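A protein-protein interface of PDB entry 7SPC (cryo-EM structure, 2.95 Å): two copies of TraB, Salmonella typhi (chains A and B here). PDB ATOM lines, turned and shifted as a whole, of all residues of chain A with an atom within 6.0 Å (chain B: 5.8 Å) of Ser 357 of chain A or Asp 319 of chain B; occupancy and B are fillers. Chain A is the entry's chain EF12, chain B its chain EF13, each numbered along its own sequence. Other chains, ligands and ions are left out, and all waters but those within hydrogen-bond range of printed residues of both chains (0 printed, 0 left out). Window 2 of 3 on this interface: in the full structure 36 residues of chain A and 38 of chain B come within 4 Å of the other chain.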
ATOM      1  N   ASP A 319     -22.764  -0.960 -22.282  1.00  0.00           N
ATOM      2  CA  ASP A 319     -21.766  -0.701 -23.359  1.00  0.00           C
ATOM      3  C   ASP A 319     -22.318   0.166 -24.500  1.00  0.00           C
ATOM      4  O   ASP A 319     -21.583   1.064 -24.908  1.00  0.00           O
ATOM      5  CB  ASP A 319     -21.197  -1.980 -23.970  1.00  0.00           C
ATOM      6  CG  ASP A 319     -19.780  -1.839 -24.485  1.00  0.00           C
ATOM      7  OD1 ASP A 319     -19.547  -1.004 -25.375  1.00  0.00           O
ATOM      8  OD2 ASP A 319     -18.924  -2.570 -23.987  1.00  0.00           O
ATOM      9  N   VAL A 355     -20.117   4.131 -20.220  1.00  0.00           N
ATOM     10  CA  VAL A 355     -19.252   3.004 -19.756  1.00  0.00           C
ATOM     11  C   VAL A 355     -19.159   1.963 -20.879  1.00  0.00           C
ATOM     12  O   VAL A 355     -20.219   1.550 -21.395  1.00  0.00           O
ATOM     13  CB  VAL A 355     -19.781   2.395 -18.442  1.00  0.00           C
ATOM     14  CG1 VAL A 355     -21.296   2.240 -18.440  1.00  0.00           C
ATOM     15  CG2 VAL A 355     -19.099   1.081 -18.094  1.00  0.00           C
ATOM     16  N   SER A 356     -17.938   1.570 -21.259  1.00  0.00           N
ATOM     17  CA  SER A 356     -17.775   0.613 -22.349  1.00  0.00           C
ATOM     18  C   SER A 356     -16.745  -0.461 -22.017  1.00  0.00           C
ATOM     19  O   SER A 356     -16.968  -1.644 -22.290  1.00  0.00           O
ATOM     20  CB  SER A 356     -17.391   1.348 -23.634  1.00  0.00           C
ATOM     21  OG  SER A 356     -18.412   2.249 -24.030  1.00  0.00           O
ATOM     22  N   SER A 357     -15.613  -0.074 -21.427  1.00  0.00           N
ATOM     23  CA  SER A 357     -14.591  -1.062 -21.091  1.00  0.00           C
ATOM     24  C   SER A 357     -15.085  -2.020 -20.014  1.00  0.00           C
ATOM     25  O   SER A 357     -14.973  -3.247 -20.150  1.00  0.00           O
ATOM     26  CB  SER A 357     -13.309  -0.359 -20.643  1.00  0.00           C
ATOM     27  OG  SER A 357     -12.317  -1.297 -20.269  1.00  0.00           O
ATOM     28  N   ALA A 358     -15.642  -1.472 -18.928  1.00  0.00           N
ATOM     29  CA  ALA A 358     -16.173  -2.311 -17.863  1.00  0.00           C
ATOM     30  C   ALA A 358     -17.333  -3.162 -18.361  1.00  0.00           C
ATOM     31  O   ALA A 358     -17.437  -4.347 -18.018  1.00  0.00           O
ATOM     32  CB  ALA A 358     -16.615  -1.444 -16.685  1.00  0.00           C
ATOM     33  N   ALA A 359     -18.212  -2.575 -19.175  1.00  0.00           N
ATOM     34  CA  ALA A 359     -19.338  -3.325 -19.719  1.00  0.00           C
ATOM     35  C   ALA A 359     -18.860  -4.479 -20.590  1.00  0.00           C
ATOM     36  O   ALA A 359     -19.395  -5.586 -20.506  1.00  0.00           O
ATOM     37  CB  ALA A 359     -20.258  -2.398 -20.510  1.00  0.00           C
ATOM     38  N   LYS A 360     -17.845  -4.242 -21.425  1.00  0.00           N
ATOM     39  CA  LYS A 360     -17.322  -5.304 -22.280  1.00  0.00           C
ATOM     40  C   LYS A 360     -16.684  -6.417 -21.457  1.00  0.00           C
ATOM     41  O   LYS A 360     -16.893  -7.607 -21.732  1.00  0.00           O
ATOM     42  CB  LYS A 360     -16.314  -4.725 -23.275  1.00  0.00           C
ATOM     43  CG  LYS A 360     -16.831  -4.638 -24.701  1.00  0.00           C
ATOM     44  CD  LYS A 360     -15.805  -4.009 -25.628  1.00  0.00           C
ATOM     45  CE  LYS A 360     -16.452  -3.516 -26.912  1.00  0.00           C
ATOM     46  NZ  LYS A 360     -15.773  -2.309 -27.454  1.00  0.00           N
ATOM     47  N   THR A 361     -15.896  -6.053 -20.440  1.00  0.00           N
ATOM     48  CA  THR A 361     -15.253  -7.071 -19.612  1.00  0.00           C
ATOM     49  C   THR A 361     -16.292  -7.916 -18.881  1.00  0.00           C
ATOM     50  O   THR A 361     -16.210  -9.154 -18.862  1.00  0.00           O
ATOM     51  CB  THR A 361     -14.300  -6.411 -18.615  1.00  0.00           C
ATOM     52  OG1 THR A 361     -14.989  -5.369 -17.913  1.00  0.00           O
ATOM     53  CG2 THR A 361     -13.099  -5.821 -19.337  1.00  0.00           C
ATOM     54  N   LEU A 362     -17.288  -7.260 -18.284  1.00  0.00           N
ATOM     55  CA  LEU A 362     -18.341  -7.988 -17.594  1.00  0.00           C
ATOM     56  C   LEU A 362     -19.159  -8.839 -18.555  1.00  0.00           C
ATOM     57  O   LEU A 362     -19.559  -9.951 -18.202  1.00  0.00           O
ATOM     58  CB  LEU A 362     -19.246  -7.017 -16.838  1.00  0.00           C
ATOM     59  CG  LEU A 362     -18.580  -6.265 -15.685  1.00  0.00           C
ATOM     60  CD1 LEU A 362     -19.576  -5.335 -15.018  1.00  0.00           C
ATOM     61  CD2 LEU A 362     -17.983  -7.238 -14.684  1.00  0.00           C
ATOM     62  N   GLY B 314     -16.656  -1.600 -11.516  1.00  0.00           N
ATOM     63  CA  GLY B 314     -16.452  -0.178 -11.216  1.00  0.00           C
ATOM     64  C   GLY B 314     -15.198   0.339 -11.874  1.00  0.00           C
ATOM     65  O   GLY B 314     -15.211   1.496 -12.314  1.00  0.00           O
ATOM     66  N   ALA B 315     -14.152  -0.481 -11.912  1.00  0.00           N
ATOM     67  CA  ALA B 315     -12.880  -0.069 -12.533  1.00  0.00           C
ATOM     68  C   ALA B 315     -13.161   0.321 -13.982  1.00  0.00           C
ATOM     69  O   ALA B 315     -12.797   1.434 -14.398  1.00  0.00           O
ATOM     70  CB  ALA B 315     -11.874  -1.178 -12.447  1.00  0.00           C
ATOM     71  N   GLY B 316     -13.839  -0.532 -14.739  1.00  0.00           N
ATOM     72  CA  GLY B 316     -14.024  -0.072 -16.126  1.00  0.00           C
ATOM     73  C   GLY B 316     -15.126   0.973 -16.306  1.00  0.00           C
ATOM     74  O   GLY B 316     -15.243   1.492 -17.438  1.00  0.00           O
ATOM     75  N   PHE B 317     -16.046   1.136 -15.346  1.00  0.00           N
ATOM     76  CA  PHE B 317     -17.035   2.245 -15.441  1.00  0.00           C
ATOM     77  C   PHE B 317     -16.217   3.524 -15.372  1.00  0.00           C
ATOM     78  O   PHE B 317     -16.435   4.507 -16.162  1.00  0.00           O
ATOM     79  CB  PHE B 317     -18.045   2.156 -14.302  1.00  0.00           C
ATOM     80  CG  PHE B 317     -19.134   3.200 -14.277  1.00  0.00           C
ATOM     81  CD1 PHE B 317     -20.259   3.069 -15.075  1.00  0.00           C
ATOM     82  CD2 PHE B 317     -19.058   4.284 -13.418  1.00  0.00           C
ATOM     83  CE1 PHE B 317     -21.268   4.019 -15.042  1.00  0.00           C
ATOM     84  CE2 PHE B 317     -20.070   5.229 -13.382  1.00  0.00           C
ATOM     85  CZ  PHE B 317     -21.172   5.098 -14.196  1.00  0.00           C
ATOM     86  N   LEU B 318     -15.233   3.469 -14.486  1.00  0.00           N
ATOM     87  CA  LEU B 318     -14.308   4.600 -14.422  1.00  0.00           C
ATOM     88  C   LEU B 318     -13.631   4.699 -15.787  1.00  0.00           C
ATOM     89  O   LEU B 318     -13.654   5.802 -16.336  1.00  0.00           O
ATOM     90  CB  LEU B 318     -13.303   4.357 -13.299  1.00  0.00           C
ATOM     91  CG  LEU B 318     -13.845   4.567 -11.889  1.00  0.00           C
ATOM     92  CD1 LEU B 318     -12.719   4.534 -10.871  1.00  0.00           C
ATOM     93  CD2 LEU B 318     -14.612   5.878 -11.796  1.00  0.00           C
ATOM     94  N   ASP B 319     -13.150   3.597 -16.354  1.00  0.00           N
ATOM     95  CA  ASP B 319     -12.566   3.659 -17.725  1.00  0.00           C
ATOM     96  C   ASP B 319     -13.480   4.361 -18.740  1.00  0.00           C
ATOM     97  O   ASP B 319     -12.938   5.163 -19.498  1.00  0.00           O
ATOM     98  CB  ASP B 319     -12.204   2.285 -18.285  1.00  0.00           C
ATOM     99  CG  ASP B 319     -11.037   2.302 -19.250  1.00  0.00           C
ATOM    100  OD1 ASP B 319     -11.127   2.985 -20.284  1.00  0.00           O
ATOM    101  OD2 ASP B 319     -10.051   1.628 -18.954  1.00  0.00           O
ATOM    102  N   GLY B 320     -14.770   4.020 -18.826  1.00  0.00           N
ATOM    103  CA  GLY B 320     -15.648   4.628 -19.836  1.00  0.00           C
ATOM    104  C   GLY B 320     -15.828   6.111 -19.595  1.00  0.00           C
ATOM    105  O   GLY B 320     -15.707   6.927 -20.576  1.00  0.00           O
ATOM    106  N   ILE B 321     -16.049   6.498 -18.338  1.00  0.00           N
ATOM    107  CA  ILE B 321     -16.126   7.973 -18.116  1.00  0.00           C
ATOM    108  C   ILE B 321     -14.804   8.609 -18.562  1.00  0.00           C
ATOM    109  O   ILE B 321     -14.860   9.690 -19.170  1.00  0.00           O
ATOM    110  CB  ILE B 321     -16.447   8.284 -16.643  1.00  0.00           C
ATOM    111  CG1 ILE B 321     -17.720   7.578 -16.178  1.00  0.00           C
ATOM    112  CG2 ILE B 321     -16.524   9.783 -16.403  1.00  0.00           C
ATOM    113  CD1 ILE B 321     -18.045   7.823 -14.724  1.00  0.00           C
ATOM    114  N   GLY B 322     -13.669   7.985 -18.234  1.00  0.00           N
ATOM    115  CA  GLY B 322     -12.329   8.489 -18.583  1.00  0.00           C
ATOM    116  C   GLY B 322     -12.180   8.672 -20.072  1.00  0.00           C
ATOM    117  O   GLY B 322     -11.667   9.720 -20.474  1.00  0.00           O
ATOM    118  N   LYS B 323     -12.645   7.715 -20.870  1.00  0.00           N
ATOM    119  CA  LYS B 323     -12.589   7.827 -22.356  1.00  0.00           C
ATOM    120  C   LYS B 323     -13.488   8.976 -22.811  1.00  0.00           C
ATOM    121  O   LYS B 323     -13.042   9.690 -23.668  1.00  0.00           O
ATOM    122  CB  LYS B 323     -12.933   6.487 -23.029  1.00  0.00           C
ATOM    123  CG  LYS B 323     -12.273   6.273 -24.386  1.00  0.00           C
ATOM    124  CD  LYS B 323     -10.764   6.369 -24.335  1.00  0.00           C
ATOM    125  CE  LYS B 323     -10.111   5.201 -23.623  1.00  0.00           C
ATOM    126  NZ  LYS B 323      -8.666   5.432 -23.407  1.00  0.00           N
ATOM    127  N   GLY B 324     -14.609   9.200 -22.138  1.00  0.00           N
ATOM    128  CA  GLY B 324     -15.578  10.228 -22.567  1.00  0.00           C
ATOM    129  C   GLY B 324     -15.210  11.566 -21.994  1.00  0.00           C
ATOM    130  O   GLY B 324     -16.068  12.467 -22.041  1.00  0.00           O
ATOM    131  N   VAL B 355     -10.075   8.855 -16.075  1.00  0.00           N
ATOM    132  CA  VAL B 355      -9.084   7.783 -15.754  1.00  0.00           C
ATOM    133  C   VAL B 355      -9.343   6.583 -16.672  1.00  0.00           C
ATOM    134  O   VAL B 355     -10.506   6.131 -16.743  1.00  0.00           O
ATOM    135  CB  VAL B 355      -9.140   7.397 -14.262  1.00  0.00           C
ATOM    136  CG1 VAL B 355     -10.566   7.292 -13.741  1.00  0.00           C
ATOM    137  CG2 VAL B 355      -8.356   6.130 -13.959  1.00  0.00           C
ATOM    138  N   SER B 356      -8.308   6.098 -17.366  1.00  0.00           N
ATOM    139  CA  SER B 356      -8.492   4.984 -18.289  1.00  0.00           C
ATOM    140  C   SER B 356      -7.389   3.941 -18.153  1.00  0.00           C
ATOM    141  O   SER B 356      -7.665   2.737 -18.154  1.00  0.00           O
ATOM    142  CB  SER B 356      -8.566   5.504 -19.726  1.00  0.00           C
ATOM    143  OG  SER B 356      -9.678   6.367 -19.898  1.00  0.00           O
ATOM    144  N   SER B 357      -6.133   4.376 -18.033  1.00  0.00           N
ATOM    145  CA  SER B 357      -5.039   3.418 -17.903  1.00  0.00           C
ATOM    146  C   SER B 357      -5.133   2.650 -16.590  1.00  0.00           C
ATOM    147  O   SER B 357      -5.047   1.413 -16.567  1.00  0.00           O
ATOM    148  CB  SER B 357      -3.695   4.140 -18.012  1.00  0.00           C
ATOM    149  OG  SER B 357      -2.616   3.238 -17.845  1.00  0.00           O
ATOM    150  N   ALA B 359      -7.800   2.327 -14.700  1.00  0.00           N
ATOM    151  CA  ALA B 359      -9.026   1.539 -14.724  1.00  0.00           C
ATOM    152  C   ALA B 359      -8.837   0.252 -15.516  1.00  0.00           C
ATOM    153  O   ALA B 359      -9.293  -0.812 -15.094  1.00  0.00           O
ATOM    154  CB  ALA B 359     -10.173   2.364 -15.302  1.00  0.00           C
ATOM    155  N   LYS B 360      -8.159   0.328 -16.664  1.00  0.00           N
ATOM    156  CA  LYS B 360      -7.924  -0.867 -17.470  1.00  0.00           C
ATOM    157  C   LYS B 360      -7.028  -1.862 -16.741  1.00  0.00           C
ATOM    158  O   LYS B 360      -7.293  -3.073 -16.747  1.00  0.00           O
ATOM    159  CB  LYS B 360      -7.310  -0.476 -18.816  1.00  0.00           C
ATOM    160  CG  LYS B 360      -8.268  -0.589 -19.990  1.00  0.00           C
ATOM    161  CD  LYS B 360      -7.616  -0.140 -21.286  1.00  0.00           C
ATOM    162  CE  LYS B 360      -8.658   0.174 -22.346  1.00  0.00           C
ATOM    163  NZ  LYS B 360      -8.218   1.263 -23.259  1.00  0.00           N
ATOM    164  N   SER B 363      -9.020  -3.419 -13.973  1.00  0.00           N
ATOM    165  CA  SER B 363     -10.010  -4.327 -14.539  1.00  0.00           C
ATOM    166  C   SER B 363      -9.376  -5.652 -14.924  1.00  0.00           C
ATOM    167  O   SER B 363      -9.925  -6.716 -14.630  1.00  0.00           O
ATOM    168  CB  SER B 363     -10.678  -3.690 -15.754  1.00  0.00           C
ATOM    169  OG  SER B 363     -11.591  -2.679 -15.372  1.00  0.00           O
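N of Ala 358 of chain A sits close to O of Gly 316 of chain B, 3.3 Å away.
Of chain B, only Asp 319 (3.7 Å) comes within 4 Å of Ser 357 of chain A.
Asp 319 of chain B touches one residue of chain A.
Printed residues of chain B within 4 Å of Val 355 of chain A: Gly 316, Phe 317 and Gly 320.
Of the printed residues of chain B, Ala 358 of chain A touches Gly 316 (2.9 Å) and Phe 317 (3.0 Å).
Printed residues of chain A within 4 Å of Phe 317 of chain B: Val 355 and Ala 358.
Printed residues of chain A within 4 Å of Gly 316 of chain B: Val 355 and Ala 358.
Of the printed residues of chain A, Gly 320 of chain B touches Val 355.
Lys 323 of chain B touches none of the printed residues of chain A.
Ser 357 of chain B touches none of the printed residues of chain A.
The nearest residue of chain A that does not touch Asp 319 of chain B is Ala 358 of chain A (5.1 Å).
The backbone carbonyl oxygen of Ala 358 of chain A lies within hydrogen-bond range of the side-chain hydroxyl of Thr 361 of chain A (2.7 Å).
N of Gly 316 of chain B is in hydrogen-bond range of OG of Ser 363 of chain B, 3.2 Å away.
The backbone NH (N) of Lys 360 of chain B sits close to the side-chain carboxylate (OD2) of Asp 319 of chain B (3.2 Å).
O of Ser 357 of chain A lies within hydrogen-bond range of OG1 of Thr 361 of chain A, 3.1 Å away.
The backbone carbonyl oxygen of Asp 319 of chain B sits at hydrogen-bond distance from the side-chain hydroxyl of Ser 356 of chain B (3.5 Å).
Ser 357 of chain A touches Asp 319 of chain B, but with the chains exchanged Asp 319 of chain A does not touch Ser 357 of chain B (15.7 Å).
6 positions are printed for both chains.
Of the 6 pairs that touch across the chains among the printed residues, none has its exchanged pair printed and touching as well.
Of the 9 printed residues of chain A, 3 touch a printed residue of chain B.
Hydrophobic or aromatic side chains of chain A within 4 Å of the printed part of chain B: Val 355 and Ala 358.
Of the 17 printed residues of chain B, 4 touch a printed residue of chain A.
Hydrophobic or aromatic side chains of chain B that line the printed part of chain A: Phe 317.
Along chain B the printed residues that touch a printed residue of chain A span positions 316 to 320.
Among the printed residues, 6 pairs touch across the chains.
Among the printed residues, merely in contact across the chains: Ala 358 of chain A with Phe 317 of chain B, Val 355 of chain A with Phe 317 of chain B, Ser 357 of chain A with Asp 319 of chain B, Val 355 of chain A with Gly 316 of chain B and Val 355 of chain A with Gly 320 of chain B.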
